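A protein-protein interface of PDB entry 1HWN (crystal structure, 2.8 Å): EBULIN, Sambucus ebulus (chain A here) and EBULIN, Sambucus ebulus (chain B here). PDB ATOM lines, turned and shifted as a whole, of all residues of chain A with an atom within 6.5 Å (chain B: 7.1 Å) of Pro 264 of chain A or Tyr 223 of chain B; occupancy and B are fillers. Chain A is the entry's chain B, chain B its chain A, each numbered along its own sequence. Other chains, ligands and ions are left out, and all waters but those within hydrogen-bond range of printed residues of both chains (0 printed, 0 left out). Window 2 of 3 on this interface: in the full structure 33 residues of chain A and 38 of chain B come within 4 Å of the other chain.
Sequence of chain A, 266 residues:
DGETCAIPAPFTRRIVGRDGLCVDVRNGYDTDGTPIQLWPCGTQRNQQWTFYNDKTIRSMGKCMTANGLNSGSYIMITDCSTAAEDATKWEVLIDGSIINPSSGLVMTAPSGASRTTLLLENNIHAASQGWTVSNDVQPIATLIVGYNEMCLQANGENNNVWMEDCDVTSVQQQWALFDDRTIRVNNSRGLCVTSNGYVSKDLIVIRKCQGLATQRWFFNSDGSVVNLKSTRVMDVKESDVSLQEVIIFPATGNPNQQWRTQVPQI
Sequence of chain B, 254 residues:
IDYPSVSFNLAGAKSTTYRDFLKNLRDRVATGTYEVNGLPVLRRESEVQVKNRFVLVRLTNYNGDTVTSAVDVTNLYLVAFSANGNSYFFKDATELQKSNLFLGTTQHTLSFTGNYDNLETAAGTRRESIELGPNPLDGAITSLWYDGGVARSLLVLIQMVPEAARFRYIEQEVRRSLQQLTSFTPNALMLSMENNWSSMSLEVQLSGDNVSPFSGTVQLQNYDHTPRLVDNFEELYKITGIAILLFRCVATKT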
ATOM      1  N   ILE A 140      32.950  -7.336 -24.679  1.00  0.00           N
ATOM      2  CA  ILE A 140      32.181  -8.323 -25.431  1.00  0.00           C
ATOM      3  C   ILE A 140      33.007  -8.966 -26.544  1.00  0.00           C
ATOM      4  O   ILE A 140      33.709  -8.279 -27.287  1.00  0.00           O
ATOM      5  CB  ILE A 140      30.919  -7.678 -26.054  1.00  0.00           C
ATOM      6  CG1 ILE A 140      29.951  -7.257 -24.946  1.00  0.00           C
ATOM      7  CG2 ILE A 140      30.238  -8.656 -26.997  1.00  0.00           C
ATOM      8  CD1 ILE A 140      29.779  -5.757 -24.817  1.00  0.00           C
ATOM      9  N   ALA A 141      32.919 -10.289 -26.649  1.00  0.00           N
ATOM     10  CA  ALA A 141      33.638 -11.037 -27.674  1.00  0.00           C
ATOM     11  C   ALA A 141      32.647 -11.459 -28.756  1.00  0.00           C
ATOM     12  O   ALA A 141      31.728 -12.235 -28.491  1.00  0.00           O
ATOM     13  CB  ALA A 141      34.298 -12.264 -27.059  1.00  0.00           C
ATOM     14  N   THR A 142      32.834 -10.952 -29.969  1.00  0.00           N
ATOM     15  CA  THR A 142      31.928 -11.277 -31.063  1.00  0.00           C
ATOM     16  C   THR A 142      32.511 -11.005 -32.444  1.00  0.00           C
ATOM     17  O   THR A 142      33.517 -10.307 -32.581  1.00  0.00           O
ATOM     18  CB  THR A 142      30.611 -10.487 -30.928  1.00  0.00           C
ATOM     19  OG1 THR A 142      29.929 -10.470 -32.186  1.00  0.00           O
ATOM     20  CG2 THR A 142      30.890  -9.059 -30.492  1.00  0.00           C
ATOM     21  N   LEU A 143      31.868 -11.564 -33.465  1.00  0.00           N
ATOM     22  CA  LEU A 143      32.300 -11.379 -34.843  1.00  0.00           C
ATOM     23  C   LEU A 143      31.517 -10.233 -35.471  1.00  0.00           C
ATOM     24  O   LEU A 143      30.581  -9.710 -34.870  1.00  0.00           O
ATOM     25  CB  LEU A 143      32.071 -12.661 -35.645  1.00  0.00           C
ATOM     26  CG  LEU A 143      32.552 -13.960 -34.992  1.00  0.00           C
ATOM     27  CD1 LEU A 143      31.383 -14.917 -34.835  1.00  0.00           C
ATOM     28  CD2 LEU A 143      33.649 -14.582 -35.838  1.00  0.00           C
ATOM     29  N   VAL A 168      34.220 -18.912 -37.265  1.00  0.00           N
ATOM     30  CA  VAL A 168      34.119 -18.774 -35.816  1.00  0.00           C
ATOM     31  C   VAL A 168      35.335 -19.327 -35.070  1.00  0.00           C
ATOM     32  O   VAL A 168      35.807 -18.721 -34.105  1.00  0.00           O
ATOM     33  CB  VAL A 168      32.843 -19.471 -35.290  1.00  0.00           C
ATOM     34  CG1 VAL A 168      32.849 -20.939 -35.695  1.00  0.00           C
ATOM     35  CG2 VAL A 168      32.751 -19.326 -33.779  1.00  0.00           C
ATOM     36  N   GLN A 262      27.883 -10.519 -33.990  1.00  0.00           N
ATOM     37  CA  GLN A 262      27.234 -11.788 -33.677  1.00  0.00           C
ATOM     38  C   GLN A 262      27.855 -12.605 -32.546  1.00  0.00           C
ATOM     39  O   GLN A 262      28.251 -13.750 -32.759  1.00  0.00           O
ATOM     40  CB  GLN A 262      27.162 -12.650 -34.939  1.00  0.00           C
ATOM     41  CG  GLN A 262      25.849 -12.538 -35.689  1.00  0.00           C
ATOM     42  CD  GLN A 262      24.665 -12.933 -34.831  1.00  0.00           C
ATOM     43  OE1 GLN A 262      24.820 -13.604 -33.812  1.00  0.00           O
ATOM     44  NE2 GLN A 262      23.473 -12.516 -35.237  1.00  0.00           N
ATOM     45  N   VAL A 263      27.914 -12.025 -31.348  1.00  0.00           N
ATOM     46  CA  VAL A 263      28.459 -12.697 -30.162  1.00  0.00           C
ATOM     47  C   VAL A 263      29.693 -13.560 -30.458  1.00  0.00           C
ATOM     48  O   VAL A 263      30.208 -13.542 -31.574  1.00  0.00           O
ATOM     49  CB  VAL A 263      27.367 -13.562 -29.473  1.00  0.00           C
ATOM     50  CG1 VAL A 263      26.599 -12.718 -28.467  1.00  0.00           C
ATOM     51  CG2 VAL A 263      26.422 -14.150 -30.504  1.00  0.00           C
ATOM     52  N   PRO A 264      30.203 -14.305 -29.456  1.00  0.00           N
ATOM     53  CA  PRO A 264      31.381 -15.149 -29.686  1.00  0.00           C
ATOM     54  C   PRO A 264      31.459 -15.745 -31.091  1.00  0.00           C
ATOM     55  O   PRO A 264      30.438 -16.294 -31.551  1.00  0.00           O
ATOM     56  CB  PRO A 264      31.270 -16.236 -28.609  1.00  0.00           C
ATOM     57  CG  PRO A 264      30.109 -15.827 -27.711  1.00  0.00           C
ATOM     58  CD  PRO A 264      29.751 -14.412 -28.059  1.00  0.00           C
ATOM     59  N   TYR B 169      19.665 -10.161 -34.197  1.00  0.00           N
ATOM     60  CA  TYR B 169      20.503 -11.315 -33.891  1.00  0.00           C
ATOM     61  C   TYR B 169      19.893 -12.573 -34.493  1.00  0.00           C
ATOM     62  O   TYR B 169      20.575 -13.349 -35.164  1.00  0.00           O
ATOM     63  CB  TYR B 169      20.644 -11.479 -32.374  1.00  0.00           C
ATOM     64  CG  TYR B 169      21.250 -12.798 -31.938  1.00  0.00           C
ATOM     65  CD1 TYR B 169      22.617 -12.914 -31.684  1.00  0.00           C
ATOM     66  CD2 TYR B 169      20.451 -13.927 -31.756  1.00  0.00           C
ATOM     67  CE1 TYR B 169      23.172 -14.120 -31.257  1.00  0.00           C
ATOM     68  CE2 TYR B 169      20.996 -15.136 -31.330  1.00  0.00           C
ATOM     69  CZ  TYR B 169      22.354 -15.226 -31.082  1.00  0.00           C
ATOM     70  OH  TYR B 169      22.886 -16.421 -30.654  1.00  0.00           O
ATOM     71  N   GLU B 173      21.025 -15.128 -37.764  1.00  0.00           N
ATOM     72  CA  GLU B 173      21.054 -16.539 -37.401  1.00  0.00           C
ATOM     73  C   GLU B 173      20.312 -17.356 -38.452  1.00  0.00           C
ATOM     74  O   GLU B 173      20.767 -18.428 -38.856  1.00  0.00           O
ATOM     75  CB  GLU B 173      20.412 -16.744 -36.028  1.00  0.00           C
ATOM     76  CG  GLU B 173      21.384 -16.630 -34.868  1.00  0.00           C
ATOM     77  CD  GLU B 173      22.722 -17.277 -35.164  1.00  0.00           C
ATOM     78  OE1 GLU B 173      23.762 -16.636 -34.909  1.00  0.00           O
ATOM     79  OE2 GLU B 173      22.733 -18.426 -35.654  1.00  0.00           O
ATOM     80  N   ASN B 187      19.346 -21.090 -28.947  1.00  0.00           N
ATOM     81  CA  ASN B 187      20.261 -21.314 -27.835  1.00  0.00           C
ATOM     82  C   ASN B 187      19.792 -20.541 -26.609  1.00  0.00           C
ATOM     83  O   ASN B 187      18.826 -19.778 -26.678  1.00  0.00           O
ATOM     84  CB  ASN B 187      21.680 -20.882 -28.216  1.00  0.00           C
ATOM     85  CG  ASN B 187      21.697 -19.640 -29.084  1.00  0.00           C
ATOM     86  OD1 ASN B 187      21.389 -18.543 -28.619  1.00  0.00           O
ATOM     87  ND2 ASN B 187      22.066 -19.805 -30.348  1.00  0.00           N
ATOM     88  N   ALA B 188      20.475 -20.743 -25.487  1.00  0.00           N
ATOM     89  CA  ALA B 188      20.126 -20.062 -24.248  1.00  0.00           C
ATOM     90  C   ALA B 188      20.018 -18.553 -24.455  1.00  0.00           C
ATOM     91  O   ALA B 188      19.135 -17.903 -23.895  1.00  0.00           O
ATOM     92  CB  ALA B 188      21.163 -20.372 -23.176  1.00  0.00           C
ATOM     93  N   LEU B 189      20.918 -18.000 -25.263  1.00  0.00           N
ATOM     94  CA  LEU B 189      20.913 -16.567 -25.534  1.00  0.00           C
ATOM     95  C   LEU B 189      19.703 -16.173 -26.368  1.00  0.00           C
ATOM     96  O   LEU B 189      18.804 -15.486 -25.886  1.00  0.00           O
ATOM     97  CB  LEU B 189      22.195 -16.154 -26.263  1.00  0.00           C
ATOM     98  CG  LEU B 189      22.246 -14.698 -26.733  1.00  0.00           C
ATOM     99  CD1 LEU B 189      22.094 -13.771 -25.537  1.00  0.00           C
ATOM    100  CD2 LEU B 189      23.556 -14.430 -27.456  1.00  0.00           C
ATOM    101  N   MET B 190      19.682 -16.616 -27.622  1.00  0.00           N
ATOM    102  CA  MET B 190      18.587 -16.314 -28.534  1.00  0.00           C
ATOM    103  C   MET B 190      17.228 -16.451 -27.861  1.00  0.00           C
ATOM    104  O   MET B 190      16.324 -15.653 -28.100  1.00  0.00           O
ATOM    105  CB  MET B 190      18.643 -17.243 -29.746  1.00  0.00           C
ATOM    106  CG  MET B 190      17.961 -16.686 -30.982  1.00  0.00           C
ATOM    107  SD  MET B 190      16.755 -17.828 -31.677  1.00  0.00           S
ATOM    108  CE  MET B 190      17.136 -17.699 -33.417  1.00  0.00           C
ATOM    109  N   MET B 193      16.861 -13.616 -24.947  1.00  0.00           N
ATOM    110  CA  MET B 193      16.726 -12.299 -25.551  1.00  0.00           C
ATOM    111  C   MET B 193      15.339 -12.066 -26.135  1.00  0.00           C
ATOM    112  O   MET B 193      14.918 -10.924 -26.311  1.00  0.00           O
ATOM    113  CB  MET B 193      17.785 -12.114 -26.640  1.00  0.00           C
ATOM    114  CG  MET B 193      17.447 -12.761 -27.972  1.00  0.00           C
ATOM    115  SD  MET B 193      18.508 -12.138 -29.287  1.00  0.00           S
ATOM    116  CE  MET B 193      20.112 -12.650 -28.686  1.00  0.00           C
ATOM    117  N   GLN B 221      20.959 -14.440 -21.058  1.00  0.00           N
ATOM    118  CA  GLN B 221      21.741 -15.649 -20.819  1.00  0.00           C
ATOM    119  C   GLN B 221      22.737 -15.954 -21.933  1.00  0.00           C
ATOM    120  O   GLN B 221      22.502 -15.639 -23.100  1.00  0.00           O
ATOM    121  CB  GLN B 221      20.809 -16.850 -20.638  1.00  0.00           C
ATOM    122  CG  GLN B 221      19.733 -16.653 -19.583  1.00  0.00           C
ATOM    123  CD  GLN B 221      19.725 -17.757 -18.543  1.00  0.00           C
ATOM    124  OE1 GLN B 221      18.720 -17.976 -17.866  1.00  0.00           O
ATOM    125  NE2 GLN B 221      20.843 -18.458 -18.409  1.00  0.00           N
ATOM    126  N   ASN B 222      23.854 -16.569 -21.559  1.00  0.00           N
ATOM    127  CA  ASN B 222      24.889 -16.935 -22.517  1.00  0.00           C
ATOM    128  C   ASN B 222      24.618 -18.340 -23.036  1.00  0.00           C
ATOM    129  O   ASN B 222      23.686 -19.003 -22.591  1.00  0.00           O
ATOM    130  CB  ASN B 222      26.268 -16.891 -21.855  1.00  0.00           C
ATOM    131  CG  ASN B 222      26.576 -15.542 -21.235  1.00  0.00           C
ATOM    132  OD1 ASN B 222      26.052 -15.198 -20.177  1.00  0.00           O
ATOM    133  ND2 ASN B 222      27.429 -14.768 -21.896  1.00  0.00           N
ATOM    134  N   TYR B 223      25.439 -18.792 -23.975  1.00  0.00           N
ATOM    135  CA  TYR B 223      25.272 -20.122 -24.545  1.00  0.00           C
ATOM    136  C   TYR B 223      25.407 -21.205 -23.477  1.00  0.00           C
ATOM    137  O   TYR B 223      24.776 -22.257 -23.569  1.00  0.00           O
ATOM    138  CB  TYR B 223      26.297 -20.344 -25.659  1.00  0.00           C
ATOM    139  CG  TYR B 223      26.088 -19.438 -26.853  1.00  0.00           C
ATOM    140  CD1 TYR B 223      27.102 -18.590 -27.300  1.00  0.00           C
ATOM    141  CD2 TYR B 223      24.868 -19.416 -27.528  1.00  0.00           C
ATOM    142  CE1 TYR B 223      26.905 -17.744 -28.394  1.00  0.00           C
ATOM    143  CE2 TYR B 223      24.662 -18.576 -28.620  1.00  0.00           C
ATOM    144  CZ  TYR B 223      25.682 -17.744 -29.047  1.00  0.00           C
ATOM    145  OH  TYR B 223      25.478 -16.918 -30.127  1.00  0.00           O
ATOM    146  N   ASP B 224      26.223 -20.940 -22.459  1.00  0.00           N
ATOM    147  CA  ASP B 224      26.428 -21.896 -21.374  1.00  0.00           C
ATOM    148  C   ASP B 224      25.405 -21.711 -20.256  1.00  0.00           C
ATOM    149  O   ASP B 224      25.608 -22.175 -19.134  1.00  0.00           O
ATOM    150  CB  ASP B 224      27.846 -21.763 -20.804  1.00  0.00           C
ATOM    151  CG  ASP B 224      28.263 -20.322 -20.609  1.00  0.00           C
ATOM    152  OD1 ASP B 224      27.371 -19.462 -20.448  1.00  0.00           O
ATOM    153  OD2 ASP B 224      29.483 -20.049 -20.617  1.00  0.00           O
ATOM    154  N   HIS B 225      24.306 -21.036 -20.577  1.00  0.00           N
ATOM    155  CA  HIS B 225      23.234 -20.783 -19.619  1.00  0.00           C
ATOM    156  C   HIS B 225      23.661 -19.878 -18.469  1.00  0.00           C
ATOM    157  O   HIS B 225      22.935 -19.716 -17.488  1.00  0.00           O
ATOM    158  CB  HIS B 225      22.707 -22.110 -19.066  1.00  0.00           C
ATOM    159  CG  HIS B 225      22.162 -23.023 -20.119  1.00  0.00           C
ATOM    160  ND1 HIS B 225      22.934 -23.969 -20.757  1.00  0.00           N
ATOM    161  CD2 HIS B 225      20.921 -23.130 -20.651  1.00  0.00           C
ATOM    162  CE1 HIS B 225      22.198 -24.615 -21.643  1.00  0.00           C
ATOM    163  NE2 HIS B 225      20.971 -24.126 -21.597  1.00  0.00           N
ATOM    164  N   THR B 226      24.843 -19.283 -18.599  1.00  0.00           N
ATOM    165  CA  THR B 226      25.376 -18.383 -17.580  1.00  0.00           C
ATOM    166  C   THR B 226      24.671 -17.026 -17.641  1.00  0.00           C
ATOM    167  O   THR B 226      24.470 -16.471 -18.722  1.00  0.00           O
ATOM    168  CB  THR B 226      26.901 -18.197 -17.775  1.00  0.00           C
ATOM    169  OG1 THR B 226      27.603 -19.008 -16.823  1.00  0.00           O
ATOM    170  CG2 THR B 226      27.306 -16.740 -17.594  1.00  0.00           C
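O of Tyr 169 of chain B lies within hydrogen-bond range of NE2 of Gln 262 of chain A, 3.0 Å away.
The side-chain amide oxygen of Gln 262 of chain A sits close to the side-chain carboxylate of Glu 173 of chain B, 3.4 Å away.
OH of Tyr 169 of chain B is in hydrogen-bond range of OD1 of Asn 187 of chain B, 3.3 Å away.
The side-chain hydroxyl (OH) of Tyr 169 of chain B is in hydrogen-bond range of the side-chain hydroxyl (OH) of Tyr 223 of chain B, 2.7 Å away.
N of Leu 189 of chain B sits close to OD1 of Asn 187 of chain B.
OG1 of Thr 142 of chain A sits at hydrogen-bond distance from N of Gln 262 of chain A (2.7 Å).
O of Leu 143 of chain A sits at hydrogen-bond distance from N of Gln 262 of chain A.
The backbone carbonyl oxygen (O) of Val 263 of chain A lies within hydrogen-bond range of the backbone NH (N) of Leu 143 of chain A (3.2 Å).
Val 263 of chain A touches Tyr 169 of chain B (CG2 to CE1, 3.3 Å).
CD2 of Leu 189 of chain B touches CG1 of Val 263 of chain A, 3.6 Å away.
Val 263 of chain A touches Tyr 223 of chain B (CG2 to OH, 2.9 Å).
CG of Pro 264 of chain A touches CE1 of Tyr 223 of chain B, 3.8 Å away.
Of the printed residues of chain B, Gln 262 of chain A touches Tyr 169 and Glu 173.
Of the printed residues of chain B, Val 263 of chain A touches Tyr 169, Leu 189 and Tyr 223.
Pro 264 of chain A touches one residue of chain B.
Of the printed residues of chain A, Glu 173 of chain B touches Gln 262 (3.4 Å).
Asn 187 of chain B touches none of the printed residues of chain A.
Printed residues of chain A within 4 Å of Leu 189 of chain B: Val 263.
Met 190 of chain B touches none of the printed residues of chain A.
Tyr 223 of chain B touches just these residues of chain A: Val 263 (2.9 Å) and Pro 264 (3.8 Å).
The nearest printed residue of chain A that does not touch Glu 173 of chain B is Val 263 of chain A (5.7 Å).
Hydrophobic or aromatic side chains of chain A within 4 Å of the printed part of chain B: Val 263 and Pro 264.
Of the 13 printed residues of chain B, 4 touch a printed residue of chain A.
Hydrophobic or aromatic side chains of chain B that line the printed part of chain A: Tyr 169, Leu 189 and Tyr 223.
Among the printed residues, 6 pairs touch across the chains.
Among the printed residues, no Asp or Glu carboxylate lies within 4 Å of a Lys or Arg side-chain nitrogen of the other chain.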
